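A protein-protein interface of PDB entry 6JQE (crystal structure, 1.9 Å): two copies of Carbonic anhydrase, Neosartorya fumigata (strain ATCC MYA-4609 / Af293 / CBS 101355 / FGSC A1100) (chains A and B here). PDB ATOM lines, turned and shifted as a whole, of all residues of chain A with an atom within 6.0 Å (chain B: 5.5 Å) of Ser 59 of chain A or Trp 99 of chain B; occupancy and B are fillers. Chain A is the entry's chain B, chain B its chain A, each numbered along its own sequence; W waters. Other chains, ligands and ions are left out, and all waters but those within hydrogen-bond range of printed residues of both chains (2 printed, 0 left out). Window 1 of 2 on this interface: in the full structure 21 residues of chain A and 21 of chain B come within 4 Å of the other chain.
The backbone NH (N) of Cys 60 of chain A is in hydrogen-bond range of the side-chain carboxylate (OD1) of Asp 57 of chain A (3.0 Å). OG1 of Thr 63 of chain A is in hydrogen-bond range of O of Ser 59 of chain A.
Water W1 lies within hydrogen-bond range of the backbone carbonyl oxygen (O) of Ala 62 of chain A (2.6 Å) and the backbone NH (N) of Gln 96 of chain B (3.1 Å). Water W2 bridges N of Leu 50 of chain B (2.8 Å) and OG1 of Thr 63 of chain A (3.2 Å).
Of the 18 printed residues of chain B, 6 touch a printed residue of chain A. Printed residues of chain B that touch a printed residue of chain A: Tyr 47, Leu 50, Asp 57, Ser 59, Gln 96 and Trp 99. Along chain B the printed residues that touch a printed residue of chain A span positions 47 to 99. Hydrophobic or aromatic side chains of chain A that line the printed part of chain B: Tyr 47, Leu 58 and Ala 62.
Tyr 47 of chain A touches its own counterpart, Tyr 47 of chain B. Tyr 47 of chain A touches Ser 59 of chain B, and with the chains exchanged Ser 59 of chain A touches Tyr 47 of chain B. Asp 57 of chain A touches its own counterpart, Asp 57 of chain B. Ser 59 of chain B touches its own counterpart, Ser 59 of chain A. 4 positions are printed for both chains. Of the 14 pairs that touch across the chains among the printed residues, 7 have their exchanged pair printed and touching as well.
Of the printed residues of chain B, Ser 59 of chain A touches Tyr 47, Asp 57, Ser 59 and Trp 99. Trp 99 of chain B touches just these residues of chain A: Leu 58 (3.6 Å), Ser 59 (3.6 Å) and Ala 62 (3.3 Å). Printed residues of chain B within 4 Å of Ala 62 of chain A: Leu 50 (3.8 Å), Gln 96 (3.5 Å) and Trp 99 (3.3 Å). Printed residues of chain B within 4 Å of Leu 58 of chain A: Asp 57 (3.1 Å) and Trp 99 (3.6 Å). Of the printed residues of chain A, Leu 50 of chain B touches Ala 62 (3.8 Å). Leu 103 of chain B touches none of the printed residues of chain A. Leu 95 of chain B touches none of the printed residues of chain A. The nearest residue of chain B that does not touch Ser 59 of chain A is Cys 60 of chain B (4.3 Å).
The side-chain carboxylate of Asp 57 of chain A sits close to the side-chain carboxylate of Asp 57 of chain B (3.1 Å). The backbone NH (N) of Ser 59 of chain B sits at hydrogen-bond distance from the side-chain carboxylate (OD2) of Asp 57 of chain A (3.0 Å). OD1 of Asp 57 of chain B lies within hydrogen-bond range of N of Leu 58 of chain A (3.1 Å). OG of Ser 59 of chain A is in hydrogen-bond range of OD2 of Asp 57 of chain B (2.7 Å).
Among the printed residues, pairs that only touch across the chains: Ala 62 of chain A with Trp 99 of chain B (3.3 Å), Ala 62 of chain A with Gln 96 of chain B (3.5 Å), Ser 59 of chain A with Trp 99 of chain B (3.6 Å), Leu 58 of chain A with Trp 99 of chain B (3.6 Å), Tyr 47 of chain A with Tyr 47 of chain B (3.6 Å), Ser 59 of chain A with Ser 59 of chain B (3.7 Å), Lys 61 of chain A with Gln 96 of chain B (3.8 Å), Ala 62 of chain A with Leu 50 of chain B (3.8 Å), Tyr 47 of chain A with Ser 59 of chain B (3.9 Å) and Ser 59 of chain A with Tyr 47 of chain B (3.9 Å).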
ATOM      1  N   TYR A  47      -3.511  18.481 -19.929  1.00  0.00           N
ATOM      2  CA  TYR A  47      -4.711  18.545 -20.808  1.00  0.00           C
ATOM      3  C   TYR A  47      -4.332  18.033 -22.200  1.00  0.00           C
ATOM      4  O   TYR A  47      -3.414  18.616 -22.791  1.00  0.00           O
ATOM      5  CB  TYR A  47      -5.270  19.969 -20.838  1.00  0.00           C
ATOM      6  CG  TYR A  47      -6.575  20.077 -21.580  1.00  0.00           C
ATOM      7  CD1 TYR A  47      -7.711  19.454 -21.086  1.00  0.00           C
ATOM      8  CD2 TYR A  47      -6.666  20.731 -22.800  1.00  0.00           C
ATOM      9  CE1 TYR A  47      -8.919  19.500 -21.772  1.00  0.00           C
ATOM     10  CE2 TYR A  47      -7.869  20.804 -23.489  1.00  0.00           C
ATOM     11  CZ  TYR A  47      -8.988  20.160 -22.990  1.00  0.00           C
ATOM     12  OH  TYR A  47     -10.169  20.212 -23.658  1.00  0.00           O
ATOM     13  N   MET A  54      -6.666  24.824 -27.786  1.00  0.00           N
ATOM     14  CA  MET A  54      -7.690  25.320 -26.849  1.00  0.00           C
ATOM     15  C   MET A  54      -8.630  26.169 -27.697  1.00  0.00           C
ATOM     16  O   MET A  54      -8.155  27.183 -28.246  1.00  0.00           O
ATOM     17  CB  MET A  54      -7.065  26.194 -25.762  1.00  0.00           C
ATOM     18  CG  MET A  54      -6.015  25.470 -24.952  1.00  0.00           C
ATOM     19  SD  MET A  54      -6.800  24.362 -23.779  1.00  0.00           S
ATOM     20  CE  MET A  54      -6.889  25.454 -22.358  1.00  0.00           C
ATOM     21  N   ASP A  57     -14.597  26.820 -25.636  1.00  0.00           N
ATOM     22  CA  ASP A  57     -15.729  25.985 -25.187  1.00  0.00           C
ATOM     23  C   ASP A  57     -15.549  25.774 -23.686  1.00  0.00           C
ATOM     24  O   ASP A  57     -14.534  26.287 -23.120  1.00  0.00           O
ATOM     25  CB  ASP A  57     -15.761  24.671 -25.963  1.00  0.00           C
ATOM     26  CG  ASP A  57     -14.636  23.700 -25.621  1.00  0.00           C
ATOM     27  OD1 ASP A  57     -13.641  24.093 -24.924  1.00  0.00           O
ATOM     28  OD2 ASP A  57     -14.767  22.544 -26.044  1.00  0.00           O
ATOM     29  N   LEU A  58     -16.417  24.970 -23.087  1.00  0.00           N
ATOM     30  CA  LEU A  58     -16.533  24.872 -21.616  1.00  0.00           C
ATOM     31  C   LEU A  58     -15.296  24.149 -21.073  1.00  0.00           C
ATOM     32  O   LEU A  58     -14.798  24.582 -20.068  1.00  0.00           O
ATOM     33  CB  LEU A  58     -17.819  24.137 -21.231  1.00  0.00           C
ATOM     34  CG  LEU A  58     -19.132  24.862 -21.521  1.00  0.00           C
ATOM     35  CD1 LEU A  58     -20.282  24.179 -20.779  1.00  0.00           C
ATOM     36  CD2 LEU A  58     -19.049  26.349 -21.139  1.00  0.00           C
ATOM     37  N   SER A  59     -14.822  23.112 -21.758  1.00  0.00           N
ATOM     38  CA  SER A  59     -13.618  22.328 -21.400  1.00  0.00           C
ATOM     39  C   SER A  59     -12.383  23.245 -21.331  1.00  0.00           C
ATOM     40  O   SER A  59     -11.636  23.130 -20.322  1.00  0.00           O
ATOM     41  CB  SER A  59     -13.420  21.197 -22.351  1.00  0.00           C
ATOM     42  OG  SER A  59     -14.477  20.255 -22.241  1.00  0.00           O
ATOM     43  N   CYS A  60     -12.140  24.123 -22.317  1.00  0.00           N
ATOM     44  CA  CYS A  60     -10.949  25.035 -22.290  1.00  0.00           C
ATOM     45  C   CYS A  60     -11.082  25.976 -21.093  1.00  0.00           C
ATOM     46  O   CYS A  60     -10.143  26.077 -20.312  1.00  0.00           O
ATOM     47  CB  CYS A  60     -10.745  25.867 -23.558  1.00  0.00           C
ATOM     48  SG  CYS A  60      -9.819  27.430 -23.327  1.00  0.00           S
ATOM     49  N   LYS A  61     -12.237  26.597 -20.928  1.00  0.00           N
ATOM     50  CA  LYS A  61     -12.484  27.571 -19.847  1.00  0.00           C
ATOM     51  C   LYS A  61     -12.376  26.875 -18.489  1.00  0.00           C
ATOM     52  O   LYS A  61     -11.699  27.426 -17.623  1.00  0.00           O
ATOM     53  CB  LYS A  61     -13.858  28.211 -20.063  1.00  0.00           C
ATOM     54  CG  LYS A  61     -13.978  29.019 -21.352  1.00  0.00           C
ATOM     55  CD  LYS A  61     -15.407  29.122 -21.867  1.00  0.00           C
ATOM     56  CE  LYS A  61     -15.496  29.552 -23.316  1.00  0.00           C
ATOM     57  NZ  LYS A  61     -16.821  30.145 -23.624  1.00  0.00           N
ATOM     58  N   ALA A  62     -13.001  25.705 -18.297  1.00  0.00           N
ATOM     59  CA  ALA A  62     -13.010  25.017 -16.988  1.00  0.00           C
ATOM     60  C   ALA A  62     -11.594  24.566 -16.643  1.00  0.00           C
ATOM     61  O   ALA A  62     -11.225  24.658 -15.451  1.00  0.00           O
ATOM     62  CB  ALA A  62     -13.961  23.853 -16.971  1.00  0.00           C
ATOM     63  N   THR A  63     -10.832  24.081 -17.626  1.00  0.00           N
ATOM     64  CA  THR A  63      -9.467  23.543 -17.369  1.00  0.00           C
ATOM     65  C   THR A  63      -8.565  24.714 -16.978  1.00  0.00           C
ATOM     66  O   THR A  63      -7.875  24.642 -15.956  1.00  0.00           O
ATOM     67  CB  THR A  63      -8.887  22.794 -18.565  1.00  0.00           C
ATOM     68  OG1 THR A  63      -9.817  21.786 -18.915  1.00  0.00           O
ATOM     69  CG2 THR A  63      -7.547  22.153 -18.279  1.00  0.00           C
ATOM     70  N   LEU A  64      -8.590  25.771 -17.781  1.00  0.00           N
ATOM     71  CA  LEU A  64      -7.820  27.001 -17.499  1.00  0.00           C
ATOM     72  C   LEU A  64      -8.178  27.496 -16.104  1.00  0.00           C
ATOM     73  O   LEU A  64      -7.251  27.705 -15.297  1.00  0.00           O
ATOM     74  CB  LEU A  64      -8.164  28.063 -18.536  1.00  0.00           C
ATOM     75  CG  LEU A  64      -7.266  29.286 -18.531  1.00  0.00           C
ATOM     76  CD1 LEU A  64      -5.792  28.903 -18.475  1.00  0.00           C
ATOM     77  CD2 LEU A  64      -7.549  30.122 -19.775  1.00  0.00           C
ATOM     78  N   TYR B  47      -7.356  11.248 -24.585  1.00  0.00           N
ATOM     79  CA  TYR B  47      -8.097  12.468 -24.189  1.00  0.00           C
ATOM     80  C   TYR B  47      -7.952  12.596 -22.669  1.00  0.00           C
ATOM     81  O   TYR B  47      -8.410  11.671 -21.948  1.00  0.00           O
ATOM     82  CB  TYR B  47      -9.556  12.407 -24.660  1.00  0.00           C
ATOM     83  CG  TYR B  47     -10.324  13.663 -24.338  1.00  0.00           C
ATOM     84  CD1 TYR B  47      -9.987  14.863 -24.951  1.00  0.00           C
ATOM     85  CD2 TYR B  47     -11.346  13.680 -23.397  1.00  0.00           C
ATOM     86  CE1 TYR B  47     -10.622  16.048 -24.628  1.00  0.00           C
ATOM     87  CE2 TYR B  47     -12.006  14.851 -23.066  1.00  0.00           C
ATOM     88  CZ  TYR B  47     -11.637  16.044 -23.682  1.00  0.00           C
ATOM     89  OH  TYR B  47     -12.243  17.228 -23.388  1.00  0.00           O
ATOM     90  N   LEU B  50     -10.565  17.062 -16.980  1.00  0.00           N
ATOM     91  CA  LEU B  50     -10.960  17.201 -15.558  1.00  0.00           C
ATOM     92  C   LEU B  50     -11.744  15.961 -15.124  1.00  0.00           C
ATOM     93  O   LEU B  50     -12.851  15.698 -15.657  1.00  0.00           O
ATOM     94  CB  LEU B  50     -11.798  18.467 -15.417  1.00  0.00           C
ATOM     95  CG  LEU B  50     -11.083  19.796 -15.657  1.00  0.00           C
ATOM     96  CD1 LEU B  50     -12.054  20.952 -15.409  1.00  0.00           C
ATOM     97  CD2 LEU B  50      -9.858  19.944 -14.758  1.00  0.00           C
ATOM     98  N   GLY B  51     -11.173  15.212 -14.189  1.00  0.00           N
ATOM     99  CA  GLY B  51     -11.825  14.066 -13.527  1.00  0.00           C
ATOM    100  C   GLY B  51     -12.177  12.937 -14.487  1.00  0.00           C
ATOM    101  O   GLY B  51     -13.127  12.200 -14.181  1.00  0.00           O
ATOM    102  N   MET B  53     -13.724  12.908 -17.151  1.00  0.00           N
ATOM    103  CA  MET B  53     -15.156  13.066 -17.477  1.00  0.00           C
ATOM    104  C   MET B  53     -15.311  13.385 -18.963  1.00  0.00           C
ATOM    105  O   MET B  53     -14.330  13.858 -19.603  1.00  0.00           O
ATOM    106  CB  MET B  53     -15.782  14.176 -16.641  1.00  0.00           C
ATOM    107  CG  MET B  53     -15.856  13.807 -15.210  1.00  0.00           C
ATOM    108  SD  MET B  53     -16.859  14.994 -14.311  1.00  0.00           S
ATOM    109  CE  MET B  53     -16.360  14.671 -12.631  1.00  0.00           C
ATOM    110  N   VAL B  55     -18.501  15.419 -20.637  1.00  0.00           N
ATOM    111  CA  VAL B  55     -19.723  16.217 -20.339  1.00  0.00           C
ATOM    112  C   VAL B  55     -20.256  16.597 -21.721  1.00  0.00           C
ATOM    113  O   VAL B  55     -19.487  16.367 -22.687  1.00  0.00           O
ATOM    114  CB  VAL B  55     -19.344  17.429 -19.467  1.00  0.00           C
ATOM    115  CG1 VAL B  55     -18.751  16.985 -18.137  1.00  0.00           C
ATOM    116  CG2 VAL B  55     -18.383  18.374 -20.176  1.00  0.00           C
ATOM    117  N   ASP B  57     -20.248  18.941 -24.122  1.00  0.00           N
ATOM    118  CA  ASP B  57     -19.510  20.157 -24.545  1.00  0.00           C
ATOM    119  C   ASP B  57     -18.955  19.832 -25.930  1.00  0.00           C
ATOM    120  O   ASP B  57     -18.902  18.615 -26.265  1.00  0.00           O
ATOM    121  CB  ASP B  57     -18.393  20.440 -23.537  1.00  0.00           C
ATOM    122  CG  ASP B  57     -17.589  21.698 -23.803  1.00  0.00           C
ATOM    123  OD1 ASP B  57     -18.195  22.694 -24.290  1.00  0.00           O
ATOM    124  OD2 ASP B  57     -16.366  21.687 -23.500  1.00  0.00           O
ATOM    125  N   SER B  59     -15.801  19.901 -27.031  1.00  0.00           N
ATOM    126  CA  SER B  59     -14.552  19.098 -26.934  1.00  0.00           C
ATOM    127  C   SER B  59     -14.884  17.601 -26.802  1.00  0.00           C
ATOM    128  O   SER B  59     -14.273  16.783 -27.505  1.00  0.00           O
ATOM    129  CB  SER B  59     -13.677  19.578 -25.806  1.00  0.00           C
ATOM    130  OG  SER B  59     -13.176  20.859 -26.105  1.00  0.00           O
ATOM    131  N   CYS B  60     -15.836  17.242 -25.948  1.00  0.00           N
ATOM    132  CA  CYS B  60     -16.198  15.818 -25.716  1.00  0.00           C
ATOM    133  C   CYS B  60     -16.822  15.252 -26.999  1.00  0.00           C
ATOM    134  O   CYS B  60     -16.369  14.203 -27.480  1.00  0.00           O
ATOM    135  CB  CYS B  60     -17.045  15.708 -24.454  1.00  0.00           C
ATOM    136  SG  CYS B  60     -16.153  16.368 -23.012  1.00  0.00           S
ATOM    137  N   LEU B  95     -13.639  24.346  -9.424  1.00  0.00           N
ATOM    138  CA  LEU B  95     -14.174  23.364 -10.409  1.00  0.00           C
ATOM    139  C   LEU B  95     -15.566  23.829 -10.841  1.00  0.00           C
ATOM    140  O   LEU B  95     -16.425  23.965  -9.971  1.00  0.00           O
ATOM    141  CB  LEU B  95     -14.195  21.980  -9.756  1.00  0.00           C
ATOM    142  CG  LEU B  95     -14.609  20.814 -10.641  1.00  0.00           C
ATOM    143  CD1 LEU B  95     -14.199  19.491 -10.022  1.00  0.00           C
ATOM    144  CD2 LEU B  95     -16.101  20.802 -10.823  1.00  0.00           C
ATOM    145  N   GLN B  96     -15.739  24.134 -12.130  1.00  0.00           N
ATOM    146  CA  GLN B  96     -16.967  24.760 -12.709  1.00  0.00           C
ATOM    147  C   GLN B  96     -17.985  23.685 -13.094  1.00  0.00           C
ATOM    148  O   GLN B  96     -17.631  22.488 -13.116  1.00  0.00           O
ATOM    149  CB  GLN B  96     -16.622  25.554 -13.970  1.00  0.00           C
ATOM    150  CG  GLN B  96     -15.877  26.854 -13.688  1.00  0.00           C
ATOM    151  CD  GLN B  96     -15.103  27.359 -14.887  1.00  0.00           C
ATOM    152  OE1 GLN B  96     -15.527  27.210 -16.033  1.00  0.00           O
ATOM    153  NE2 GLN B  96     -13.959  27.977 -14.626  1.00  0.00           N
ATOM    154  N   LYS B  97     -19.198  24.107 -13.432  1.00  0.00           N
ATOM    155  CA  LYS B  97     -20.270  23.218 -13.947  1.00  0.00           C
ATOM    156  C   LYS B  97     -19.948  22.972 -15.412  1.00  0.00           C
ATOM    157  O   LYS B  97     -19.355  23.844 -16.040  1.00  0.00           O
ATOM    158  CB  LYS B  97     -21.639  23.884 -13.775  1.00  0.00           C
ATOM    159  CG  LYS B  97     -22.030  24.160 -12.332  1.00  0.00           C
ATOM    160  CD  LYS B  97     -23.387  24.822 -12.164  1.00  0.00           C
ATOM    161  CE  LYS B  97     -23.503  25.548 -10.836  1.00  0.00           C
ATOM    162  NZ  LYS B  97     -24.907  25.888 -10.493  1.00  0.00           N
ATOM    163  N   PRO B  98     -20.308  21.807 -15.997  1.00  0.00           N
ATOM    164  CA  PRO B  98     -21.025  20.754 -15.284  1.00  0.00           C
ATOM    165  C   PRO B  98     -20.199  19.721 -14.491  1.00  0.00           C
ATOM    166  O   PRO B  98     -20.820  18.876 -13.881  1.00  0.00           O
ATOM    167  CB  PRO B  98     -21.778  20.083 -16.442  1.00  0.00           C
ATOM    168  CG  PRO B  98     -20.836  20.187 -17.602  1.00  0.00           C
ATOM    169  CD  PRO B  98     -20.115  21.504 -17.420  1.00  0.00           C
ATOM    170  N   TRP B  99     -18.862  19.824 -14.469  1.00  0.00           N
ATOM    171  CA  TRP B  99     -17.966  18.911 -13.696  1.00  0.00           C
ATOM    172  C   TRP B  99     -18.420  18.854 -12.239  1.00  0.00           C
ATOM    173  O   TRP B  99     -18.583  17.739 -11.691  1.00  0.00           O
ATOM    174  CB  TRP B  99     -16.491  19.328 -13.842  1.00  0.00           C
ATOM    175  CG  TRP B  99     -16.011  19.186 -15.252  1.00  0.00           C
ATOM    176  CD1 TRP B  99     -15.377  18.100 -15.766  1.00  0.00           C
ATOM    177  CD2 TRP B  99     -16.159  20.122 -16.332  1.00  0.00           C
ATOM    178  NE1 TRP B  99     -15.147  18.280 -17.099  1.00  0.00           N
ATOM    179  CE2 TRP B  99     -15.585  19.516 -17.472  1.00  0.00           C
ATOM    180  CE3 TRP B  99     -16.681  21.423 -16.455  1.00  0.00           C
ATOM    181  CZ2 TRP B  99     -15.539  20.146 -18.717  1.00  0.00           C
ATOM    182  CZ3 TRP B  99     -16.628  22.051 -17.683  1.00  0.00           C
ATOM    183  CH2 TRP B  99     -16.074  21.413 -18.802  1.00  0.00           C
ATOM    184  N   SER B 100     -18.647  20.013 -11.629  1.00  0.00           N
ATOM    185  CA  SER B 100     -19.046  20.123 -10.202  1.00  0.00           C
ATOM    186  C   SER B 100     -20.430  19.487 -10.015  1.00  0.00           C
ATOM    187  O   SER B 100     -20.634  18.883  -8.948  1.00  0.00           O
ATOM    188  CB  SER B 100     -19.055  21.555  -9.728  1.00  0.00           C
ATOM    189  OG  SER B 100     -20.030  22.287 -10.462  1.00  0.00           O
ATOM    190  N   SER B 101     -21.328  19.629 -11.001  1.00  0.00           N
ATOM    191  CA  SER B 101     -22.709  19.061 -11.000  1.00  0.00           C
ATOM    192  C   SER B 101     -22.667  17.532 -11.002  1.00  0.00           C
ATOM    193  O   SER B 101     -23.399  16.917 -10.232  1.00  0.00           O
ATOM    194  CB  SER B 101     -23.507  19.564 -12.179  1.00  0.00           C
ATOM    195  OG  SER B 101     -23.498  20.987 -12.213  1.00  0.00           O
ATOM    196  N   VAL B 102     -21.866  16.931 -11.878  1.00  0.00           N
ATOM    197  CA  VAL B 102     -21.650  15.459 -11.929  1.00  0.00           C
ATOM    198  C   VAL B 102     -21.259  14.986 -10.521  1.00  0.00           C
ATOM    199  O   VAL B 102     -21.882  14.026 -10.016  1.00  0.00           O
ATOM    200  CB  VAL B 102     -20.605  15.081 -12.994  1.00  0.00           C
ATOM    201  CG1 VAL B 102     -20.293  13.598 -12.962  1.00  0.00           C
ATOM    202  CG2 VAL B 102     -21.047  15.507 -14.386  1.00  0.00           C
ATOM    203  N   LEU B 103     -20.301  15.652  -9.874  1.00  0.00           N
ATOM    204  CA  LEU B 103     -19.756  15.172  -8.578  1.00  0.00           C
ATOM    205  C   LEU B 103     -20.818  15.349  -7.487  1.00  0.00           C
ATOM    206  O   LEU B 103     -20.991  14.421  -6.708  1.00  0.00           O
ATOM    207  CB  LEU B 103     -18.468  15.929  -8.240  1.00  0.00           C
ATOM    208  CG  LEU B 103     -17.268  15.532  -9.094  1.00  0.00           C
ATOM    209  CD1 LEU B 103     -16.100  16.458  -8.813  1.00  0.00           C
ATOM    210  CD2 LEU B 103     -16.900  14.069  -8.865  1.00  0.00           C
ATOM    211  N   ASP B 104     -21.526  16.476  -7.466  1.00  0.00           N
ATOM    212  CA  ASP B 104     -22.615  16.712  -6.489  1.00  0.00           C
ATOM    213  C   ASP B 104     -23.700  15.642  -6.684  1.00  0.00           C
ATOM    214  O   ASP B 104     -24.145  15.082  -5.682  1.00  0.00           O
ATOM    215  CB  ASP B 104     -23.194  18.126  -6.607  1.00  0.00           C
ATOM    216  CG  ASP B 104     -22.278  19.247  -6.123  1.00  0.00           C
ATOM    217  OD1 ASP B 104     -21.336  18.968  -5.336  1.00  0.00           O
ATOM    218  OD2 ASP B 104     -22.499  20.401  -6.540  1.00  0.00           O
HETATM  219  O   HOH W   1     -12.968  24.693 -13.499  1.00  0.00           O
HETATM  220  O   HOH W   2     -11.197  18.877 -19.040  1.00  0.00           O
